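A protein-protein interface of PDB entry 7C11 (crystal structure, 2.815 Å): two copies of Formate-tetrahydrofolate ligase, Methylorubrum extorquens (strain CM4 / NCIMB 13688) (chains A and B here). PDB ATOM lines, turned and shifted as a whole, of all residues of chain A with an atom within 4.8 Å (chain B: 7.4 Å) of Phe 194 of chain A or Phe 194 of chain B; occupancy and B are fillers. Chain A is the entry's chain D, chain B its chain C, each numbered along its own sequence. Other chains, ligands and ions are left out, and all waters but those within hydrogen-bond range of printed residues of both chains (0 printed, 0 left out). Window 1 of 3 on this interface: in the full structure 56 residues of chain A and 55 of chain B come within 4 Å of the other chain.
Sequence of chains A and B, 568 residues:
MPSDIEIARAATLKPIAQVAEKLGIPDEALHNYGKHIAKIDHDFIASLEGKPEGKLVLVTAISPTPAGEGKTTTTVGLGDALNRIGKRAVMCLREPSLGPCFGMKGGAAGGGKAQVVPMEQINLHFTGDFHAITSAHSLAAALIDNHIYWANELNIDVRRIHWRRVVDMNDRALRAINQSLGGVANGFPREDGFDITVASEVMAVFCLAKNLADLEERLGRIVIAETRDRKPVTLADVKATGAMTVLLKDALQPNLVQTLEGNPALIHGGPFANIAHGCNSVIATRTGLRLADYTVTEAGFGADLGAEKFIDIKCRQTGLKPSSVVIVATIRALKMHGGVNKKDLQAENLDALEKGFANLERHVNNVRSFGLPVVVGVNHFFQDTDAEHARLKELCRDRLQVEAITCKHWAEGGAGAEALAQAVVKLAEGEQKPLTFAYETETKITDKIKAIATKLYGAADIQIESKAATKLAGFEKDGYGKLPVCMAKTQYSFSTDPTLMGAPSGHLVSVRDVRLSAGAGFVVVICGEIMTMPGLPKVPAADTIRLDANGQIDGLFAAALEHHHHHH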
ATOM      1  N   ARG A 164     -22.201  19.990  22.763  1.00  0.00           N
ATOM      2  CA  ARG A 164     -21.204  18.917  22.972  1.00  0.00           C
ATOM      3  C   ARG A 164     -19.841  19.579  23.197  1.00  0.00           C
ATOM      4  O   ARG A 164     -19.773  20.825  23.231  1.00  0.00           O
ATOM      5  CB  ARG A 164     -21.144  17.976  21.770  1.00  0.00           C
ATOM      6  CG  ARG A 164     -22.472  17.398  21.306  1.00  0.00           C
ATOM      7  CD  ARG A 164     -22.167  16.412  20.194  1.00  0.00           C
ATOM      8  NE  ARG A 164     -22.051  15.083  20.763  1.00  0.00           N
ATOM      9  CZ  ARG A 164     -21.183  14.148  20.400  1.00  0.00           C
ATOM     10  NH1 ARG A 164     -21.224  12.981  21.014  1.00  0.00           N
ATOM     11  NH2 ARG A 164     -20.301  14.349  19.431  1.00  0.00           N
ATOM     12  N   ARG A 165     -18.793  18.782  23.385  1.00  0.00           N
ATOM     13  CA  ARG A 165     -17.418  19.283  23.615  1.00  0.00           C
ATOM     14  C   ARG A 165     -16.637  19.080  22.309  1.00  0.00           C
ATOM     15  O   ARG A 165     -17.232  18.573  21.354  1.00  0.00           O
ATOM     16  CB  ARG A 165     -16.788  18.548  24.812  1.00  0.00           C
ATOM     17  CG  ARG A 165     -16.978  19.245  26.144  1.00  0.00           C
ATOM     18  CD  ARG A 165     -16.856  18.320  27.340  1.00  0.00           C
ATOM     19  NE  ARG A 165     -16.852  19.144  28.538  1.00  0.00           N
ATOM     20  CZ  ARG A 165     -17.921  19.434  29.278  1.00  0.00           C
ATOM     21  NH1 ARG A 165     -19.105  18.893  29.016  1.00  0.00           N
ATOM     22  NH2 ARG A 165     -17.790  20.245  30.319  1.00  0.00           N
ATOM     23  N   VAL A 166     -15.364  19.481  22.260  1.00  0.00           N
ATOM     24  CA  VAL A 166     -14.546  19.403  21.017  1.00  0.00           C
ATOM     25  C   VAL A 166     -13.086  19.240  21.392  1.00  0.00           C
ATOM     26  O   VAL A 166     -12.687  19.618  22.511  1.00  0.00           O
ATOM     27  CB  VAL A 166     -14.696  20.632  20.095  1.00  0.00           C
ATOM     28  CG1 VAL A 166     -16.115  20.815  19.570  1.00  0.00           C
ATOM     29  CG2 VAL A 166     -14.207  21.915  20.762  1.00  0.00           C
ATOM     30  N   VAL A 167     -12.331  18.761  20.412  1.00  0.00           N
ATOM     31  CA  VAL A 167     -10.850  18.651  20.408  1.00  0.00           C
ATOM     32  C   VAL A 167     -10.492  18.461  18.948  1.00  0.00           C
ATOM     33  O   VAL A 167     -11.335  17.872  18.263  1.00  0.00           O
ATOM     34  CB  VAL A 167     -10.385  17.487  21.297  1.00  0.00           C
ATOM     35  CG1 VAL A 167     -11.222  16.245  21.068  1.00  0.00           C
ATOM     36  CG2 VAL A 167      -8.919  17.169  21.106  1.00  0.00           C
ATOM     37  N   LEU A 174     -14.099   9.654  22.266  1.00  0.00           N
ATOM     38  CA  LEU A 174     -14.799  10.783  22.935  1.00  0.00           C
ATOM     39  C   LEU A 174     -16.154  11.040  22.265  1.00  0.00           C
ATOM     40  O   LEU A 174     -16.870  11.950  22.724  1.00  0.00           O
ATOM     41  CB  LEU A 174     -13.871  12.010  22.926  1.00  0.00           C
ATOM     42  CG  LEU A 174     -12.511  11.843  23.634  1.00  0.00           C
ATOM     43  CD1 LEU A 174     -11.739  13.143  23.690  1.00  0.00           C
ATOM     44  CD2 LEU A 174     -12.668  11.275  25.042  1.00  0.00           C
ATOM     45  N   ARG A 175     -16.531  10.228  21.274  1.00  0.00           N
ATOM     46  CA  ARG A 175     -17.814  10.351  20.531  1.00  0.00           C
ATOM     47  C   ARG A 175     -18.996  10.374  21.497  1.00  0.00           C
ATOM     48  O   ARG A 175     -19.848  11.188  21.312  1.00  0.00           O
ATOM     49  CB  ARG A 175     -18.013   9.183  19.559  1.00  0.00           C
ATOM     50  CG  ARG A 175     -17.431   9.425  18.176  1.00  0.00           C
ATOM     51  CD  ARG A 175     -17.314   8.116  17.428  1.00  0.00           C
ATOM     52  NE  ARG A 175     -16.644   8.264  16.145  1.00  0.00           N
ATOM     53  CZ  ARG A 175     -16.295   7.250  15.363  1.00  0.00           C
ATOM     54  NH1 ARG A 175     -16.525   6.000  15.739  1.00  0.00           N
ATOM     55  NH2 ARG A 175     -15.691   7.488  14.212  1.00  0.00           N
ATOM     56  N   ILE A 177     -19.575   9.863  25.814  1.00  0.00           N
ATOM     57  CA  ILE A 177     -19.008   9.677  27.185  1.00  0.00           C
ATOM     58  C   ILE A 177     -20.134   9.803  28.219  1.00  0.00           C
ATOM     59  O   ILE A 177     -21.236  10.233  27.843  1.00  0.00           O
ATOM     60  CB  ILE A 177     -17.861  10.689  27.429  1.00  0.00           C
ATOM     61  CG1 ILE A 177     -18.380  12.131  27.468  1.00  0.00           C
ATOM     62  CG2 ILE A 177     -16.770  10.515  26.379  1.00  0.00           C
ATOM     63  CD1 ILE A 177     -17.342  13.175  27.810  1.00  0.00           C
ATOM     64  N   GLY A 193     -20.536  14.054  24.651  1.00  0.00           N
ATOM     65  CA  GLY A 193     -19.551  13.464  23.722  1.00  0.00           C
ATOM     66  C   GLY A 193     -18.695  14.568  23.160  1.00  0.00           C
ATOM     67  O   GLY A 193     -18.902  15.704  23.625  1.00  0.00           O
ATOM     68  N   PHE A 194     -17.764  14.262  22.257  1.00  0.00           N
ATOM     69  CA  PHE A 194     -16.923  15.263  21.553  1.00  0.00           C
ATOM     70  C   PHE A 194     -17.158  15.157  20.041  1.00  0.00           C
ATOM     71  O   PHE A 194     -17.392  14.060  19.559  1.00  0.00           O
ATOM     72  CB  PHE A 194     -15.437  15.106  21.883  1.00  0.00           C
ATOM     73  CG  PHE A 194     -15.002  15.528  23.272  1.00  0.00           C
ATOM     74  CD1 PHE A 194     -15.550  14.938  24.407  1.00  0.00           C
ATOM     75  CD2 PHE A 194     -13.970  16.447  23.443  1.00  0.00           C
ATOM     76  CE1 PHE A 194     -15.108  15.288  25.676  1.00  0.00           C
ATOM     77  CE2 PHE A 194     -13.514  16.774  24.705  1.00  0.00           C
ATOM     78  CZ  PHE A 194     -14.094  16.208  25.822  1.00  0.00           C
ATOM     79  N   ASP A 195     -17.197  16.300  19.352  1.00  0.00           N
ATOM     80  CA  ASP A 195     -17.021  16.433  17.883  1.00  0.00           C
ATOM     81  C   ASP A 195     -15.612  16.973  17.676  1.00  0.00           C
ATOM     82  O   ASP A 195     -15.034  17.486  18.640  1.00  0.00           O
ATOM     83  CB  ASP A 195     -18.067  17.340  17.216  1.00  0.00           C
ATOM     84  CG  ASP A 195     -19.507  16.959  17.552  1.00  0.00           C
ATOM     85  OD1 ASP A 195     -19.751  15.776  17.767  1.00  0.00           O
ATOM     86  OD2 ASP A 195     -20.380  17.864  17.625  1.00  0.00           O
ATOM     87  N   ILE A 196     -15.073  16.803  16.479  1.00  0.00           N
ATOM     88  CA  ILE A 196     -13.800  17.449  16.063  1.00  0.00           C
ATOM     89  C   ILE A 196     -14.067  18.958  16.006  1.00  0.00           C
ATOM     90  O   ILE A 196     -15.177  19.356  15.619  1.00  0.00           O
ATOM     91  CB  ILE A 196     -13.294  16.852  14.726  1.00  0.00           C
ATOM     92  CG1 ILE A 196     -11.812  17.158  14.490  1.00  0.00           C
ATOM     93  CG2 ILE A 196     -14.144  17.297  13.537  1.00  0.00           C
ATOM     94  CD1 ILE A 196     -11.147  16.151  13.585  1.00  0.00           C
ATOM     95  N   MET A 533     -16.746  13.156  14.407  1.00  0.00           N
ATOM     96  CA  MET A 533     -15.485  12.726  15.058  1.00  0.00           C
ATOM     97  C   MET A 533     -14.961  11.509  14.302  1.00  0.00           C
ATOM     98  O   MET A 533     -15.485  10.405  14.462  1.00  0.00           O
ATOM     99  CB  MET A 533     -15.710  12.387  16.530  1.00  0.00           C
ATOM    100  CG  MET A 533     -14.477  11.828  17.192  1.00  0.00           C
ATOM    101  SD  MET A 533     -13.036  12.912  17.139  1.00  0.00           S
ATOM    102  CE  MET A 533     -13.491  14.058  18.434  1.00  0.00           C
ATOM    103  N   SER B 138      -3.075  14.737  23.818  1.00  0.00           N
ATOM    104  CA  SER B 138      -4.403  14.324  23.300  1.00  0.00           C
ATOM    105  C   SER B 138      -4.260  13.318  22.145  1.00  0.00           C
ATOM    106  O   SER B 138      -5.238  12.537  21.914  1.00  0.00           O
ATOM    107  CB  SER B 138      -5.223  15.534  22.936  1.00  0.00           C
ATOM    108  OG  SER B 138      -5.556  16.288  24.114  1.00  0.00           O
ATOM    109  N   ARG B 164      -4.217   9.615  31.478  1.00  0.00           N
ATOM    110  CA  ARG B 164      -5.518  10.331  31.504  1.00  0.00           C
ATOM    111  C   ARG B 164      -5.472  11.340  30.360  1.00  0.00           C
ATOM    112  O   ARG B 164      -4.421  11.485  29.729  1.00  0.00           O
ATOM    113  CB  ARG B 164      -5.726  11.014  32.864  1.00  0.00           C
ATOM    114  CG  ARG B 164      -5.870  10.047  34.032  1.00  0.00           C
ATOM    115  CD  ARG B 164      -5.776  10.653  35.416  1.00  0.00           C
ATOM    116  NE  ARG B 164      -6.653  11.808  35.642  1.00  0.00           N
ATOM    117  CZ  ARG B 164      -7.948  11.759  35.980  1.00  0.00           C
ATOM    118  NH1 ARG B 164      -8.637  12.873  36.175  1.00  0.00           N
ATOM    119  NH2 ARG B 164      -8.553  10.592  36.115  1.00  0.00           N
ATOM    120  N   ARG B 165      -6.553  12.046  30.110  1.00  0.00           N
ATOM    121  CA  ARG B 165      -6.532  13.060  29.052  1.00  0.00           C
ATOM    122  C   ARG B 165      -6.330  14.422  29.707  1.00  0.00           C
ATOM    123  O   ARG B 165      -6.144  14.452  30.956  1.00  0.00           O
ATOM    124  CB  ARG B 165      -7.803  12.931  28.231  1.00  0.00           C
ATOM    125  CG  ARG B 165      -7.713  11.871  27.144  1.00  0.00           C
ATOM    126  CD  ARG B 165      -9.099  11.345  26.866  1.00  0.00           C
ATOM    127  NE  ARG B 165      -9.103  10.775  25.545  1.00  0.00           N
ATOM    128  CZ  ARG B 165      -8.875   9.500  25.242  1.00  0.00           C
ATOM    129  NH1 ARG B 165      -8.897   9.114  23.975  1.00  0.00           N
ATOM    130  NH2 ARG B 165      -8.630   8.609  26.195  1.00  0.00           N
ATOM    131  N   VAL B 166      -6.313  15.483  28.882  1.00  0.00           N
ATOM    132  CA  VAL B 166      -6.063  16.881  29.313  1.00  0.00           C
ATOM    133  C   VAL B 166      -6.837  17.859  28.438  1.00  0.00           C
ATOM    134  O   VAL B 166      -6.972  17.651  27.203  1.00  0.00           O
ATOM    135  CB  VAL B 166      -4.564  17.246  29.274  1.00  0.00           C
ATOM    136  CG1 VAL B 166      -3.752  16.444  30.281  1.00  0.00           C
ATOM    137  CG2 VAL B 166      -3.959  17.159  27.880  1.00  0.00           C
ATOM    138  N   VAL B 167      -7.184  18.968  29.069  1.00  0.00           N
ATOM    139  CA  VAL B 167      -7.666  20.223  28.431  1.00  0.00           C
ATOM    140  C   VAL B 167      -7.131  21.351  29.311  1.00  0.00           C
ATOM    141  O   VAL B 167      -6.916  21.046  30.529  1.00  0.00           O
ATOM    142  CB  VAL B 167      -9.204  20.227  28.358  1.00  0.00           C
ATOM    143  CG1 VAL B 167      -9.832  19.728  29.661  1.00  0.00           C
ATOM    144  CG2 VAL B 167      -9.744  21.607  27.998  1.00  0.00           C
ATOM    145  N   ASP B 168      -6.933  22.575  28.773  1.00  0.00           N
ATOM    146  CA  ASP B 168      -6.440  23.720  29.599  1.00  0.00           C
ATOM    147  C   ASP B 168      -7.634  24.516  30.150  1.00  0.00           C
ATOM    148  O   ASP B 168      -7.773  25.689  29.862  1.00  0.00           O
ATOM    149  CB  ASP B 168      -5.389  24.544  28.855  1.00  0.00           C
ATOM    150  CG  ASP B 168      -4.529  25.425  29.754  1.00  0.00           C
ATOM    151  OD1 ASP B 168      -4.330  25.068  30.937  1.00  0.00           O
ATOM    152  OD2 ASP B 168      -4.036  26.459  29.251  1.00  0.00           O
ATOM    153  N   MET B 169      -8.482  23.871  30.942  1.00  0.00           N
ATOM    154  CA  MET B 169      -9.723  24.474  31.496  1.00  0.00           C
ATOM    155  C   MET B 169      -9.948  23.858  32.880  1.00  0.00           C
ATOM    156  O   MET B 169      -9.552  22.703  33.080  1.00  0.00           O
ATOM    157  CB  MET B 169     -10.937  24.245  30.587  1.00  0.00           C
ATOM    158  CG  MET B 169     -10.910  25.096  29.316  1.00  0.00           C
ATOM    159  SD  MET B 169     -11.598  26.733  29.640  1.00  0.00           S
ATOM    160  CE  MET B 169     -10.458  27.813  28.800  1.00  0.00           C
ATOM    161  N   ASP B 171     -12.163  22.240  34.421  1.00  0.00           N
ATOM    162  CA  ASP B 171     -13.444  21.543  34.122  1.00  0.00           C
ATOM    163  C   ASP B 171     -13.650  20.310  35.007  1.00  0.00           C
ATOM    164  O   ASP B 171     -13.295  19.214  34.612  1.00  0.00           O
ATOM    165  CB  ASP B 171     -13.616  21.172  32.654  1.00  0.00           C
ATOM    166  CG  ASP B 171     -15.067  20.843  32.324  1.00  0.00           C
ATOM    167  OD1 ASP B 171     -15.948  21.054  33.227  1.00  0.00           O
ATOM    168  OD2 ASP B 171     -15.313  20.402  31.159  1.00  0.00           O
ATOM    169  N   ARG B 172     -14.352  20.519  36.108  1.00  0.00           N
ATOM    170  CA  ARG B 172     -14.739  19.532  37.135  1.00  0.00           C
ATOM    171  C   ARG B 172     -15.512  18.378  36.504  1.00  0.00           C
ATOM    172  O   ARG B 172     -15.382  17.239  36.993  1.00  0.00           O
ATOM    173  CB  ARG B 172     -15.582  20.302  38.158  1.00  0.00           C
ATOM    174  CG  ARG B 172     -16.403  19.454  39.118  1.00  0.00           C
ATOM    175  CD  ARG B 172     -17.510  20.278  39.767  1.00  0.00           C
ATOM    176  NE  ARG B 172     -17.047  21.459  40.474  1.00  0.00           N
ATOM    177  CZ  ARG B 172     -17.235  22.705  40.080  1.00  0.00           C
ATOM    178  NH1 ARG B 172     -16.793  23.692  40.834  1.00  0.00           N
ATOM    179  NH2 ARG B 172     -17.872  22.976  38.956  1.00  0.00           N
ATOM    180  N   ALA B 173     -16.305  18.653  35.476  1.00  0.00           N
ATOM    181  CA  ALA B 173     -17.165  17.644  34.804  1.00  0.00           C
ATOM    182  C   ALA B 173     -16.331  16.443  34.306  1.00  0.00           C
ATOM    183  O   ALA B 173     -16.895  15.338  34.262  1.00  0.00           O
ATOM    184  CB  ALA B 173     -17.914  18.309  33.671  1.00  0.00           C
ATOM    185  N   LEU B 174     -15.056  16.653  33.926  1.00  0.00           N
ATOM    186  CA  LEU B 174     -14.202  15.651  33.232  1.00  0.00           C
ATOM    187  C   LEU B 174     -13.227  14.948  34.201  1.00  0.00           C
ATOM    188  O   LEU B 174     -12.499  14.050  33.720  1.00  0.00           O
ATOM    189  CB  LEU B 174     -13.449  16.308  32.058  1.00  0.00           C
ATOM    190  CG  LEU B 174     -14.293  16.989  30.964  1.00  0.00           C
ATOM    191  CD1 LEU B 174     -13.398  17.693  29.932  1.00  0.00           C
ATOM    192  CD2 LEU B 174     -15.260  16.032  30.259  1.00  0.00           C
ATOM    193  N   ARG B 175     -13.190  15.278  35.497  1.00  0.00           N
ATOM    194  CA  ARG B 175     -12.327  14.541  36.468  1.00  0.00           C
ATOM    195  C   ARG B 175     -12.577  13.030  36.401  1.00  0.00           C
ATOM    196  O   ARG B 175     -11.612  12.281  36.512  1.00  0.00           O
ATOM    197  CB  ARG B 175     -12.600  14.934  37.914  1.00  0.00           C
ATOM    198  CG  ARG B 175     -12.023  16.278  38.307  1.00  0.00           C
ATOM    199  CD  ARG B 175     -12.693  16.648  39.616  1.00  0.00           C
ATOM    200  NE  ARG B 175     -12.367  17.997  40.045  1.00  0.00           N
ATOM    201  CZ  ARG B 175     -13.029  18.673  40.957  1.00  0.00           C
ATOM    202  NH1 ARG B 175     -14.080  18.145  41.562  1.00  0.00           N
ATOM    203  NH2 ARG B 175     -12.612  19.884  41.261  1.00  0.00           N
ATOM    204  N   ALA B 176     -13.826  12.592  36.260  1.00  0.00           N
ATOM    205  CA  ALA B 176     -14.161  11.159  36.134  1.00  0.00           C
ATOM    206  C   ALA B 176     -15.189  10.945  35.002  1.00  0.00           C
ATOM    207  O   ALA B 176     -16.270  11.510  35.053  1.00  0.00           O
ATOM    208  CB  ALA B 176     -14.596  10.618  37.493  1.00  0.00           C
ATOM    209  N   ILE B 177     -14.859  10.079  34.052  1.00  0.00           N
ATOM    210  CA  ILE B 177     -15.508   9.922  32.720  1.00  0.00           C
ATOM    211  C   ILE B 177     -15.702   8.428  32.470  1.00  0.00           C
ATOM    212  O   ILE B 177     -14.908   7.619  32.997  1.00  0.00           O
ATOM    213  CB  ILE B 177     -14.584  10.562  31.650  1.00  0.00           C
ATOM    214  CG1 ILE B 177     -14.570  12.092  31.739  1.00  0.00           C
ATOM    215  CG2 ILE B 177     -14.837  10.073  30.229  1.00  0.00           C
ATOM    216  CD1 ILE B 177     -15.898  12.721  31.586  1.00  0.00           C
ATOM    217  N   GLN B 179     -15.815   6.605  28.755  1.00  0.00           N
ATOM    218  CA  GLN B 179     -15.561   6.872  27.315  1.00  0.00           C
ATOM    219  C   GLN B 179     -15.709   5.584  26.491  1.00  0.00           C
ATOM    220  O   GLN B 179     -15.996   4.508  27.074  1.00  0.00           O
ATOM    221  CB  GLN B 179     -14.170   7.465  27.160  1.00  0.00           C
ATOM    222  CG  GLN B 179     -13.105   6.590  27.775  1.00  0.00           C
ATOM    223  CD  GLN B 179     -11.925   6.347  26.868  1.00  0.00           C
ATOM    224  OE1 GLN B 179     -11.961   5.509  25.964  1.00  0.00           O
ATOM    225  NE2 GLN B 179     -10.852   7.074  27.138  1.00  0.00           N
ATOM    226  N   ASP B 192     -12.304   6.730  32.510  1.00  0.00           N
ATOM    227  CA  ASP B 192     -11.254   7.707  32.143  1.00  0.00           C
ATOM    228  C   ASP B 192     -11.475   8.988  32.952  1.00  0.00           C
ATOM    229  O   ASP B 192     -12.459   9.088  33.678  1.00  0.00           O
ATOM    230  CB  ASP B 192     -11.230   7.880  30.627  1.00  0.00           C
ATOM    231  CG  ASP B 192      -9.942   8.459  30.069  1.00  0.00           C
ATOM    232  OD1 ASP B 192      -8.945   8.592  30.845  1.00  0.00           O
ATOM    233  OD2 ASP B 192      -9.952   8.783  28.857  1.00  0.00           O
ATOM    234  N   GLY B 193     -10.506   9.889  32.900  1.00  0.00           N
ATOM    235  CA  GLY B 193     -10.606  11.230  33.498  1.00  0.00           C
ATOM    236  C   GLY B 193      -9.705  12.188  32.754  1.00  0.00           C
ATOM    237  O   GLY B 193      -8.867  11.694  31.974  1.00  0.00           O
ATOM    238  N   PHE B 194      -9.892  13.485  32.983  1.00  0.00           N
ATOM    239  CA  PHE B 194      -9.070  14.600  32.462  1.00  0.00           C
ATOM    240  C   PHE B 194      -8.383  15.322  33.636  1.00  0.00           C
ATOM    241  O   PHE B 194      -9.051  15.637  34.650  1.00  0.00           O
ATOM    242  CB  PHE B 194      -9.955  15.607  31.724  1.00  0.00           C
ATOM    243  CG  PHE B 194     -10.347  15.261  30.307  1.00  0.00           C
ATOM    244  CD1 PHE B 194     -11.224  14.221  30.038  1.00  0.00           C
ATOM    245  CD2 PHE B 194      -9.882  16.025  29.235  1.00  0.00           C
ATOM    246  CE1 PHE B 194     -11.594  13.931  28.730  1.00  0.00           C
ATOM    247  CE2 PHE B 194     -10.271  15.744  27.929  1.00  0.00           C
ATOM    248  CZ  PHE B 194     -11.118  14.685  27.680  1.00  0.00           C
ATOM    249  N   ASP B 195      -7.087  15.627  33.491  1.00  0.00           N
ATOM    250  CA  ASP B 195      -6.405  16.672  34.293  1.00  0.00           C
ATOM    251  C   ASP B 195      -6.339  17.946  33.452  1.00  0.00           C
ATOM    252  O   ASP B 195      -6.690  17.913  32.254  1.00  0.00           O
ATOM    253  CB  ASP B 195      -5.056  16.178  34.781  1.00  0.00           C
ATOM    254  CG  ASP B 195      -5.181  14.826  35.461  1.00  0.00           C
ATOM    255  OD1 ASP B 195      -6.010  14.731  36.373  1.00  0.00           O
ATOM    256  OD2 ASP B 195      -4.478  13.854  35.032  1.00  0.00           O
ATOM    257  N   ILE B 196      -5.999  19.063  34.079  1.00  0.00           N
ATOM    258  CA  ILE B 196      -5.555  20.259  33.319  1.00  0.00           C
ATOM    259  C   ILE B 196      -4.252  19.911  32.566  1.00  0.00           C
ATOM    260  O   ILE B 196      -3.427  19.070  33.060  1.00  0.00           O
ATOM    261  CB  ILE B 196      -5.451  21.487  34.244  1.00  0.00           C
ATOM    262  CG1 ILE B 196      -5.482  22.788  33.433  1.00  0.00           C
ATOM    263  CG2 ILE B 196      -4.240  21.421  35.165  1.00  0.00           C
ATOM    264  CD1 ILE B 196      -6.156  23.949  34.174  1.00  0.00           C
ATOM    265  N   THR B 197      -4.089  20.489  31.374  1.00  0.00           N
ATOM    266  CA  THR B 197      -2.884  20.365  30.515  1.00  0.00           C
ATOM    267  C   THR B 197      -1.596  20.427  31.352  1.00  0.00           C
ATOM    268  O   THR B 197      -0.668  19.701  31.030  1.00  0.00           O
ATOM    269  CB  THR B 197      -2.944  21.452  29.439  1.00  0.00           C
ATOM    270  OG1 THR B 197      -3.846  20.937  28.461  1.00  0.00           O
ATOM    271  CG2 THR B 197      -1.597  21.794  28.838  1.00  0.00           C
ATOM    272  N   THR B 532      -5.679  17.475  40.453  1.00  0.00           N
ATOM    273  CA  THR B 532      -5.034  17.609  39.130  1.00  0.00           C
ATOM    274  C   THR B 532      -5.985  18.343  38.176  1.00  0.00           C
ATOM    275  O   THR B 532      -5.493  18.869  37.124  1.00  0.00           O
ATOM    276  CB  THR B 532      -4.636  16.240  38.583  1.00  0.00           C
ATOM    277  OG1 THR B 532      -5.806  15.451  38.766  1.00  0.00           O
ATOM    278  CG2 THR B 532      -3.451  15.624  39.288  1.00  0.00           C
ATOM    279  N   MET B 533      -7.287  18.385  38.508  1.00  0.00           N
ATOM    280  CA  MET B 533      -8.301  19.171  37.737  1.00  0.00           C
ATOM    281  C   MET B 533      -9.051  20.147  38.644  1.00  0.00           C
ATOM    282  O   MET B 533      -9.959  19.753  39.359  1.00  0.00           O
ATOM    283  CB  MET B 533      -9.308  18.275  37.017  1.00  0.00           C
ATOM    284  CG  MET B 533     -10.311  19.091  36.241  1.00  0.00           C
ATOM    285  SD  MET B 533      -9.602  20.294  35.032  1.00  0.00           S
ATOM    286  CE  MET B 533      -9.542  19.193  33.623  1.00  0.00           C
ATOM    287  N   PRO B 534      -8.714  21.454  38.651  1.00  0.00           N
ATOM    288  CA  PRO B 534      -9.408  22.411  39.514  1.00  0.00           C
ATOM    289  C   PRO B 534     -10.791  22.717  38.924  1.00  0.00           C
ATOM    290  O   PRO B 534     -11.020  22.369  37.795  1.00  0.00           O
ATOM    291  CB  PRO B 534      -8.500  23.647  39.529  1.00  0.00           C
ATOM    292  CG  PRO B 534      -7.881  23.581  38.145  1.00  0.00           C
ATOM    293  CD  PRO B 534      -7.651  22.100  37.874  1.00  0.00           C
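Arg 165 of chain A touches Leu 174 of chain B, and with the chains exchanged Leu 174 of chain A touches Arg 165 of chain B. Phe 194 of chain A touches its own counterpart, Phe 194 of chain B. 12 positions are printed for both chains.
Of the printed residues of chain B, Leu 174 of chain A touches Arg 165 (3.6 Å). Of the printed residues of chain A, Arg 165 of chain B touches Leu 174 (3.6 Å). Printed residues of chain A within 4 Å of Asp 171 of chain B: Arg 165. Of the printed residues of chain A, Gln 179 of chain B touches Ile 177. Gly 193 of chain B touches none of the printed residues of chain A. Of chain A, only Phe 194 (3.8 Å) comes within 4 Å of Phe 194 of chain B. The nearest printed residue of chain A that does not touch Arg 165 of chain B is Phe 194 of chain A (7.0 Å).
Printed residues of chain B that touch a printed residue of chain A: Arg 165, Asp 171, Ala 173, Leu 174, Gln 179 and Phe 194. Hydrophobic or aromatic side chains of chain B within 4 Å of the printed part of chain A: Ala 173, Leu 174 and Phe 194. Hydrophobic or aromatic side chains of chain A within 4 Å of the printed part of chain B: Leu 174, Ile 177 and Phe 194. Along chain A the printed residues that touch a printed residue of chain B span positions 165 to 194. Among the printed residues, Asp or Glu carboxylates within 4 Å of a Lys or Arg side-chain nitrogen of the other chain: Arg 165 of chain A with Asp 171 of chain B.
The side-chain carboxylate of Asp 171 of chain B lies within salt-bridge range of the guanidinium group of Arg 165 of chain A, at 2.6 Å.
NH1 of Arg 164 of chain B sits at hydrogen-bond distance from O of Phe 194 of chain B (3.2 Å). O of Leu 174 of chain B sits at hydrogen-bond distance from N of Phe 194 of chain B. The backbone carbonyl oxygen (O) of Arg 165 of chain A sits at hydrogen-bond distance from the backbone NH (N) of Asp 195 of chain A, 3.0 Å away. The backbone carbonyl oxygen (O) of Gly 193 of chain B lies within hydrogen-bond range of the backbone NH (N) of Arg 165 of chain B (3.0 Å). NE2 of Gln 179 of chain B sits at hydrogen-bond distance from OD2 of Asp 192 of chain B (2.6 Å). The backbone NH of Asp 195 of chain B sits at hydrogen-bond distance from the backbone carbonyl oxygen of Arg 165 of chain B (2.9 Å).
Arg 165 of chain A touches Ala 173 of chain B (NH2 to CB, 3.9 Å). Arg 165 of chain A touches Leu 174 of chain B (NE to CD2, 3.9 Å). Leu 174 of chain A touches Arg 165 of chain B (CD2 to NE, 3.6 Å). CG2 of Ile 177 of chain A touches CA of Gln 179 of chain B, 3.95 Å away. CZ of Phe 194 of chain A touches CZ of Phe 194 of chain B, 3.8 Å away.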
